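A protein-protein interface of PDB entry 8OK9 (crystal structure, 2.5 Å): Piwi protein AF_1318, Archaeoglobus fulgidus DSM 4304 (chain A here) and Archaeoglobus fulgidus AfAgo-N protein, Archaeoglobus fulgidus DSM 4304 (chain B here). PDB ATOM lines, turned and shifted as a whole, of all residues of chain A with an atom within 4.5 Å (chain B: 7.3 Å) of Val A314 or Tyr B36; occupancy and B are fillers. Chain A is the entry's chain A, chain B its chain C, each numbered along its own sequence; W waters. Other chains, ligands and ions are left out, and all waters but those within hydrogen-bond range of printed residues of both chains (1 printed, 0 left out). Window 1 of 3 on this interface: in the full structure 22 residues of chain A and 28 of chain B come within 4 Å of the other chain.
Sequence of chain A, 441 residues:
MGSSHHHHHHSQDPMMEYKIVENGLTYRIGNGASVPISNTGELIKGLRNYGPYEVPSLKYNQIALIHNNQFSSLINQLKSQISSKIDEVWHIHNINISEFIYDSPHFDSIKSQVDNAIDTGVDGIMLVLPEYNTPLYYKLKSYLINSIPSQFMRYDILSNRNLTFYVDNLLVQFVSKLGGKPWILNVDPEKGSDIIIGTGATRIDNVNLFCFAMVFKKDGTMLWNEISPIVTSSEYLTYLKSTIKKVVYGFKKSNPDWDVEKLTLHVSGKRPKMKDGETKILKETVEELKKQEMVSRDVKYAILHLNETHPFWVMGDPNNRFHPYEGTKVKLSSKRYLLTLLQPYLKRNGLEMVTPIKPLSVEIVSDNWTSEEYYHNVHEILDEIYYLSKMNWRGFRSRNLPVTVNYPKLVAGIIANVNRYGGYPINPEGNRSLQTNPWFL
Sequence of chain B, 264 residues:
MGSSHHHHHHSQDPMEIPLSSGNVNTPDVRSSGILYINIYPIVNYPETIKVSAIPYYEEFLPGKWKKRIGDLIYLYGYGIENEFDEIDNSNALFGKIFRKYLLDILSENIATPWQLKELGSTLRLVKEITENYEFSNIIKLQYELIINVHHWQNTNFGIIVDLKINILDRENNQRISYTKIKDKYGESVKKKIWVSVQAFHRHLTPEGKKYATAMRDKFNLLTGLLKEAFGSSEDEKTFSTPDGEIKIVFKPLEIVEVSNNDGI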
ATOM      1  N   TRP A 313      18.945 -20.413  14.786  1.00  0.00           N
ATOM      2  CA  TRP A 313      17.724 -19.620  14.810  1.00  0.00           C
ATOM      3  C   TRP A 313      18.109 -18.147  14.842  1.00  0.00           C
ATOM      4  O   TRP A 313      19.111 -17.770  15.453  1.00  0.00           O
ATOM      5  CB  TRP A 313      16.839 -19.948  16.023  1.00  0.00           C
ATOM      6  CG  TRP A 313      16.308 -21.350  16.045  1.00  0.00           C
ATOM      7  CD1 TRP A 313      16.903 -22.444  16.604  1.00  0.00           C
ATOM      8  CD2 TRP A 313      15.065 -21.807  15.497  1.00  0.00           C
ATOM      9  NE1 TRP A 313      16.111 -23.554  16.431  1.00  0.00           N
ATOM     10  CE2 TRP A 313      14.977 -23.189  15.753  1.00  0.00           C
ATOM     11  CE3 TRP A 313      14.019 -21.180  14.809  1.00  0.00           C
ATOM     12  CZ2 TRP A 313      13.886 -23.956  15.349  1.00  0.00           C
ATOM     13  CZ3 TRP A 313      12.937 -21.944  14.408  1.00  0.00           C
ATOM     14  CH2 TRP A 313      12.879 -23.317  14.679  1.00  0.00           C
ATOM     15  N   VAL A 314      17.305 -17.316  14.182  1.00  0.00           N
ATOM     16  CA  VAL A 314      17.565 -15.883  14.094  1.00  0.00           C
ATOM     17  C   VAL A 314      16.331 -15.126  14.569  1.00  0.00           C
ATOM     18  O   VAL A 314      15.221 -15.377  14.088  1.00  0.00           O
ATOM     19  CB  VAL A 314      17.946 -15.454  12.664  1.00  0.00           C
ATOM     20  CG1 VAL A 314      18.113 -13.943  12.589  1.00  0.00           C
ATOM     21  CG2 VAL A 314      19.220 -16.156  12.223  1.00  0.00           C
ATOM     22  N   MET A 315      16.530 -14.201  15.507  1.00  0.00           N
ATOM     23  CA  MET A 315      15.467 -13.383  16.073  1.00  0.00           C
ATOM     24  C   MET A 315      15.591 -11.955  15.556  1.00  0.00           C
ATOM     25  O   MET A 315      16.697 -11.412  15.476  1.00  0.00           O
ATOM     26  CB  MET A 315      15.527 -13.399  17.603  1.00  0.00           C
ATOM     27  CG  MET A 315      14.554 -12.452  18.286  1.00  0.00           C
ATOM     28  SD  MET A 315      14.361 -12.834  20.037  1.00  0.00           S
ATOM     29  CE  MET A 315      14.278 -11.189  20.740  1.00  0.00           C
ATOM     30  N   GLY A 316      14.455 -11.344  15.217  1.00  0.00           N
ATOM     31  CA  GLY A 316      14.446 -10.065  14.544  1.00  0.00           C
ATOM     32  C   GLY A 316      13.585  -9.031  15.254  1.00  0.00           C
ATOM     33  O   GLY A 316      13.449  -9.025  16.480  1.00  0.00           O
ATOM     34  N   PRO A 324      13.356 -11.969  11.638  1.00  0.00           N
ATOM     35  CA  PRO A 324      14.064 -11.190  10.619  1.00  0.00           C
ATOM     36  C   PRO A 324      13.213 -11.046   9.368  1.00  0.00           C
ATOM     37  O   PRO A 324      12.291 -11.824   9.112  1.00  0.00           O
ATOM     38  CB  PRO A 324      15.324 -12.018  10.346  1.00  0.00           C
ATOM     39  CG  PRO A 324      14.940 -13.410  10.718  1.00  0.00           C
ATOM     40  CD  PRO A 324      13.993 -13.276  11.878  1.00  0.00           C
ATOM     41  N   LEU A 338      23.203 -17.782   6.332  1.00  0.00           N
ATOM     42  CA  LEU A 338      21.831 -18.106   6.700  1.00  0.00           C
ATOM     43  C   LEU A 338      20.897 -17.145   5.980  1.00  0.00           C
ATOM     44  O   LEU A 338      21.057 -15.924   6.083  1.00  0.00           O
ATOM     45  CB  LEU A 338      21.618 -18.017   8.211  1.00  0.00           C
ATOM     46  CG  LEU A 338      22.399 -19.010   9.069  1.00  0.00           C
ATOM     47  CD1 LEU A 338      22.233 -18.681  10.543  1.00  0.00           C
ATOM     48  CD2 LEU A 338      21.959 -20.438   8.776  1.00  0.00           C
ATOM     49  N   PRO A 359      15.736 -20.135   9.339  1.00  0.00           N
ATOM     50  CA  PRO A 359      16.365 -19.751   8.068  1.00  0.00           C
ATOM     51  C   PRO A 359      16.957 -20.941   7.330  1.00  0.00           C
ATOM     52  O   PRO A 359      16.963 -22.064   7.844  1.00  0.00           O
ATOM     53  CB  PRO A 359      17.456 -18.766   8.505  1.00  0.00           C
ATOM     54  CG  PRO A 359      17.798 -19.195   9.893  1.00  0.00           C
ATOM     55  CD  PRO A 359      16.496 -19.643  10.501  1.00  0.00           C
ATOM     56  N   SER B  32      16.191  -0.181  15.526  1.00  0.00           N
ATOM     57  CA  SER B  32      17.571  -0.549  15.824  1.00  0.00           C
ATOM     58  C   SER B  32      18.168  -1.400  14.707  1.00  0.00           C
ATOM     59  O   SER B  32      19.315  -1.199  14.306  1.00  0.00           O
ATOM     60  CB  SER B  32      17.650  -1.301  17.156  1.00  0.00           C
ATOM     61  OG  SER B  32      17.237  -2.648  17.006  1.00  0.00           O
ATOM     62  N   ILE B  34      18.805  -4.661  14.870  1.00  0.00           N
ATOM     63  CA  ILE B  34      19.725  -5.643  15.430  1.00  0.00           C
ATOM     64  C   ILE B  34      19.052  -7.007  15.411  1.00  0.00           C
ATOM     65  O   ILE B  34      17.890  -7.142  15.814  1.00  0.00           O
ATOM     66  CB  ILE B  34      20.146  -5.259  16.861  1.00  0.00           C
ATOM     67  CG1 ILE B  34      20.868  -3.910  16.862  1.00  0.00           C
ATOM     68  CG2 ILE B  34      21.017  -6.346  17.477  1.00  0.00           C
ATOM     69  CD1 ILE B  34      22.310  -3.986  16.414  1.00  0.00           C
ATOM     70  N   LEU B  35      19.776  -8.017  14.940  1.00  0.00           N
ATOM     71  CA  LEU B  35      19.308  -9.393  14.957  1.00  0.00           C
ATOM     72  C   LEU B  35      20.036 -10.176  16.041  1.00  0.00           C
ATOM     73  O   LEU B  35      21.057  -9.742  16.580  1.00  0.00           O
ATOM     74  CB  LEU B  35      19.502 -10.056  13.588  1.00  0.00           C
ATOM     75  CG  LEU B  35      18.899  -9.321  12.391  1.00  0.00           C
ATOM     76  CD1 LEU B  35      19.097 -10.127  11.118  1.00  0.00           C
ATOM     77  CD2 LEU B  35      17.425  -9.025  12.622  1.00  0.00           C
ATOM     78  N   TYR B  36      19.479 -11.342  16.370  1.00  0.00           N
ATOM     79  CA  TYR B  36      20.065 -12.193  17.435  1.00  0.00           C
ATOM     80  C   TYR B  36      20.148 -13.627  16.918  1.00  0.00           C
ATOM     81  O   TYR B  36      19.262 -14.036  16.167  1.00  0.00           O
ATOM     82  CB  TYR B  36      19.223 -12.116  18.710  1.00  0.00           C
ATOM     83  CG  TYR B  36      19.216 -10.762  19.367  1.00  0.00           C
ATOM     84  CD1 TYR B  36      20.266 -10.357  20.172  1.00  0.00           C
ATOM     85  CD2 TYR B  36      18.172  -9.875  19.167  1.00  0.00           C
ATOM     86  CE1 TYR B  36      20.271  -9.112  20.776  1.00  0.00           C
ATOM     87  CE2 TYR B  36      18.166  -8.623  19.756  1.00  0.00           C
ATOM     88  CZ  TYR B  36      19.219  -8.240  20.565  1.00  0.00           C
ATOM     89  OH  TYR B  36      19.221  -7.009  21.152  1.00  0.00           O
ATOM     90  N   ILE B  37      21.197 -14.354  17.301  1.00  0.00           N
ATOM     91  CA  ILE B  37      21.369 -15.768  16.858  1.00  0.00           C
ATOM     92  C   ILE B  37      21.615 -16.618  18.105  1.00  0.00           C
ATOM     93  O   ILE B  37      22.060 -16.054  19.112  1.00  0.00           O
ATOM     94  CB  ILE B  37      22.496 -15.881  15.808  1.00  0.00           C
ATOM     95  CG1 ILE B  37      22.524 -17.239  15.105  1.00  0.00           C
ATOM     96  CG2 ILE B  37      23.850 -15.508  16.388  1.00  0.00           C
ATOM     97  CD1 ILE B  37      23.137 -17.183  13.736  1.00  0.00           C
ATOM     98  N   ASN B  38      21.339 -17.921  18.035  1.00  0.00           N
ATOM     99  CA  ASN B  38      21.508 -18.807  19.214  1.00  0.00           C
ATOM    100  C   ASN B  38      22.977 -19.217  19.331  1.00  0.00           C
ATOM    101  O   ASN B  38      23.246 -20.413  19.518  1.00  0.00           O
ATOM    102  CB  ASN B  38      20.552 -20.002  19.169  1.00  0.00           C
ATOM    103  CG  ASN B  38      20.583 -20.799  17.884  1.00  0.00           C
ATOM    104  OD1 ASN B  38      21.197 -20.400  16.897  1.00  0.00           O
ATOM    105  ND2 ASN B  38      19.921 -21.941  17.893  1.00  0.00           N
ATOM    106  N   ILE B  39      23.883 -18.240  19.278  1.00  0.00           N
ATOM    107  CA  ILE B  39      25.335 -18.505  19.456  1.00  0.00           C
ATOM    108  C   ILE B  39      25.739 -17.680  20.674  1.00  0.00           C
ATOM    109  O   ILE B  39      25.470 -16.472  20.681  1.00  0.00           O
ATOM    110  CB  ILE B  39      26.146 -18.115  18.204  1.00  0.00           C
ATOM    111  CG1 ILE B  39      25.726 -18.916  16.971  1.00  0.00           C
ATOM    112  CG2 ILE B  39      27.641 -18.238  18.463  1.00  0.00           C
ATOM    113  CD1 ILE B  39      26.482 -18.541  15.721  1.00  0.00           C
ATOM    114  N   MET B 215       8.931 -16.203  19.035  1.00  0.00           N
ATOM    115  CA  MET B 215      10.372 -16.258  18.806  1.00  0.00           C
ATOM    116  C   MET B 215      11.144 -15.654  19.975  1.00  0.00           C
ATOM    117  O   MET B 215      12.203 -16.167  20.355  1.00  0.00           O
ATOM    118  CB  MET B 215      10.728 -15.548  17.500  1.00  0.00           C
ATOM    119  CG  MET B 215      12.223 -15.486  17.226  1.00  0.00           C
ATOM    120  SD  MET B 215      12.955 -17.111  16.926  1.00  0.00           S
ATOM    121  CE  MET B 215      12.398 -17.429  15.254  1.00  0.00           C
ATOM    122  N   PHE B 219      13.729 -17.774  22.520  1.00  0.00           N
ATOM    123  CA  PHE B 219      15.104 -17.384  22.814  1.00  0.00           C
ATOM    124  C   PHE B 219      15.330 -17.234  24.314  1.00  0.00           C
ATOM    125  O   PHE B 219      16.412 -17.554  24.818  1.00  0.00           O
ATOM    126  CB  PHE B 219      15.449 -16.087  22.085  1.00  0.00           C
ATOM    127  CG  PHE B 219      16.193 -16.297  20.801  1.00  0.00           C
ATOM    128  CD1 PHE B 219      15.565 -16.875  19.708  1.00  0.00           C
ATOM    129  CD2 PHE B 219      17.520 -15.922  20.685  1.00  0.00           C
ATOM    130  CE1 PHE B 219      16.249 -17.072  18.524  1.00  0.00           C
ATOM    131  CE2 PHE B 219      18.209 -16.116  19.503  1.00  0.00           C
ATOM    132  CZ  PHE B 219      17.573 -16.692  18.421  1.00  0.00           C
ATOM    133  N   LYS B 251      24.187 -14.437  26.610  1.00  0.00           N
ATOM    134  CA  LYS B 251      23.293 -13.552  25.879  1.00  0.00           C
ATOM    135  C   LYS B 251      23.489 -13.859  24.397  1.00  0.00           C
ATOM    136  O   LYS B 251      24.642 -13.948  23.934  1.00  0.00           O
ATOM    137  CB  LYS B 251      23.553 -12.069  26.163  1.00  0.00           C
ATOM    138  CG  LYS B 251      23.737 -11.732  27.637  1.00  0.00           C
ATOM    139  CD  LYS B 251      24.468 -10.413  27.826  1.00  0.00           C
ATOM    140  CE  LYS B 251      23.518  -9.234  27.710  1.00  0.00           C
ATOM    141  NZ  LYS B 251      24.232  -7.933  27.832  1.00  0.00           N
ATOM    142  N   PRO B 252      22.407 -14.038  23.640  1.00  0.00           N
ATOM    143  CA  PRO B 252      22.547 -14.388  22.221  1.00  0.00           C
ATOM    144  C   PRO B 252      23.359 -13.350  21.459  1.00  0.00           C
ATOM    145  O   PRO B 252      23.249 -12.146  21.699  1.00  0.00           O
ATOM    146  CB  PRO B 252      21.097 -14.445  21.726  1.00  0.00           C
ATOM    147  CG  PRO B 252      20.292 -14.726  22.952  1.00  0.00           C
ATOM    148  CD  PRO B 252      21.000 -14.027  24.076  1.00  0.00           C
ATOM    149  N   LEU B 253      24.184 -13.839  20.536  1.00  0.00           N
ATOM    150  CA  LEU B 253      25.053 -12.970  19.754  1.00  0.00           C
ATOM    151  C   LEU B 253      24.233 -11.997  18.915  1.00  0.00           C
ATOM    152  O   LEU B 253      23.156 -12.335  18.413  1.00  0.00           O
ATOM    153  CB  LEU B 253      25.955 -13.813  18.854  1.00  0.00           C
ATOM    154  CG  LEU B 253      27.176 -13.156  18.217  1.00  0.00           C
ATOM    155  CD1 LEU B 253      28.214 -12.827  19.272  1.00  0.00           C
ATOM    156  CD2 LEU B 253      27.760 -14.082  17.169  1.00  0.00           C
ATOM    157  N   GLU B 254      24.747 -10.780  18.768  1.00  0.00           N
ATOM    158  CA  GLU B 254      24.083  -9.748  17.988  1.00  0.00           C
ATOM    159  C   GLU B 254      24.614  -9.738  16.560  1.00  0.00           C
ATOM    160  O   GLU B 254      25.792 -10.006  16.310  1.00  0.00           O
ATOM    161  CB  GLU B 254      24.284  -8.373  18.627  1.00  0.00           C
ATOM    162  CG  GLU B 254      23.607  -8.209  19.980  1.00  0.00           C
ATOM    163  CD  GLU B 254      23.732  -6.800  20.530  1.00  0.00           C
ATOM    164  OE1 GLU B 254      24.325  -5.942  19.843  1.00  0.00           O
ATOM    165  OE2 GLU B 254      23.236  -6.550  21.649  1.00  0.00           O
ATOM    166  N   ILE B 255      23.726  -9.430  15.618  1.00  0.00           N
ATOM    167  CA  ILE B 255      24.070  -9.337  14.203  1.00  0.00           C
ATOM    168  C   ILE B 255      23.653  -7.955  13.720  1.00  0.00           C
ATOM    169  O   ILE B 255      22.484  -7.573  13.862  1.00  0.00           O
ATOM    170  CB  ILE B 255      23.389 -10.433  13.369  1.00  0.00           C
ATOM    171  CG1 ILE B 255      23.667 -11.813  13.968  1.00  0.00           C
ATOM    172  CG2 ILE B 255      23.863 -10.380  11.924  1.00  0.00           C
ATOM    173  CD1 ILE B 255      22.478 -12.744  13.910  1.00  0.00           C
HETATM  174  O   HOH W   1      15.678  -6.845  18.026  1.00  0.00           O
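The backbone carbonyl oxygen (O) of Leu B35 lies within hydrogen-bond range of the backbone NH (N) of Ile B255 (2.9 Å). N of Ile B37 lies within hydrogen-bond range of O of Leu B253, at 3.0 Å.
N of Trp A313 lies within hydrogen-bond range of OD1 of Asn B38 (3.1 Å). The backbone carbonyl oxygen (O) of Tyr B36 sits at hydrogen-bond distance from the backbone NH (N) of Met A315 (2.8 Å).
Hydrophobic or aromatic side chains of chain A within 4 Å of the printed part of chain B: Trp A313, Val A314, Met A315 and Leu A338. Along chain B the printed residues that touch a printed residue of chain A span positions 35 to 219. Among the printed residues, 12 pairs touch across the chains. Among the printed residues, no Asp or Glu carboxylate lies within 4 Å of a Lys or Arg side-chain nitrogen of the other chain.
Water W1 lies within hydrogen-bond range of O of Ile B34 (3.1 Å) and O of Gly A316 (3.5 Å).
Among the printed residues, pairs that only touch across the chains: Val A314 with Tyr B36, Trp A313 with Ile B37, Met A315 with Leu B35, Trp A313 with Phe B219, Leu A338 with Ile B37, Val A314 with Met B215, Gly A316 with Leu B35, Trp A313 with Tyr B36, Met A315 with Phe B219 and Met A315 with Met B215.
Of the printed residues of chain B, Val A314 touches Tyr B36 (3.3 Å) and Met B215 (3.7 Å). Printed residues of chain A within 4 Å of Leu B35: Met A315 and Gly A316. Tyr B36 touches just these residues of chain A: Trp A313, Val A314 and Met A315. Printed residues of chain A within 4 Å of Ile B37: Trp A313 and Leu A338. Of the printed residues of chain A, Asn B38 touches Trp A313 (3.1 Å). Ile B255 touches none of the printed residues of chain A. The nearest residue of chain B that does not touch Val A314 is Leu B35 (4.2 Å). The nearest printed residue of chain A that does not touch Asn B38 is Val A314 (5.6 Å).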
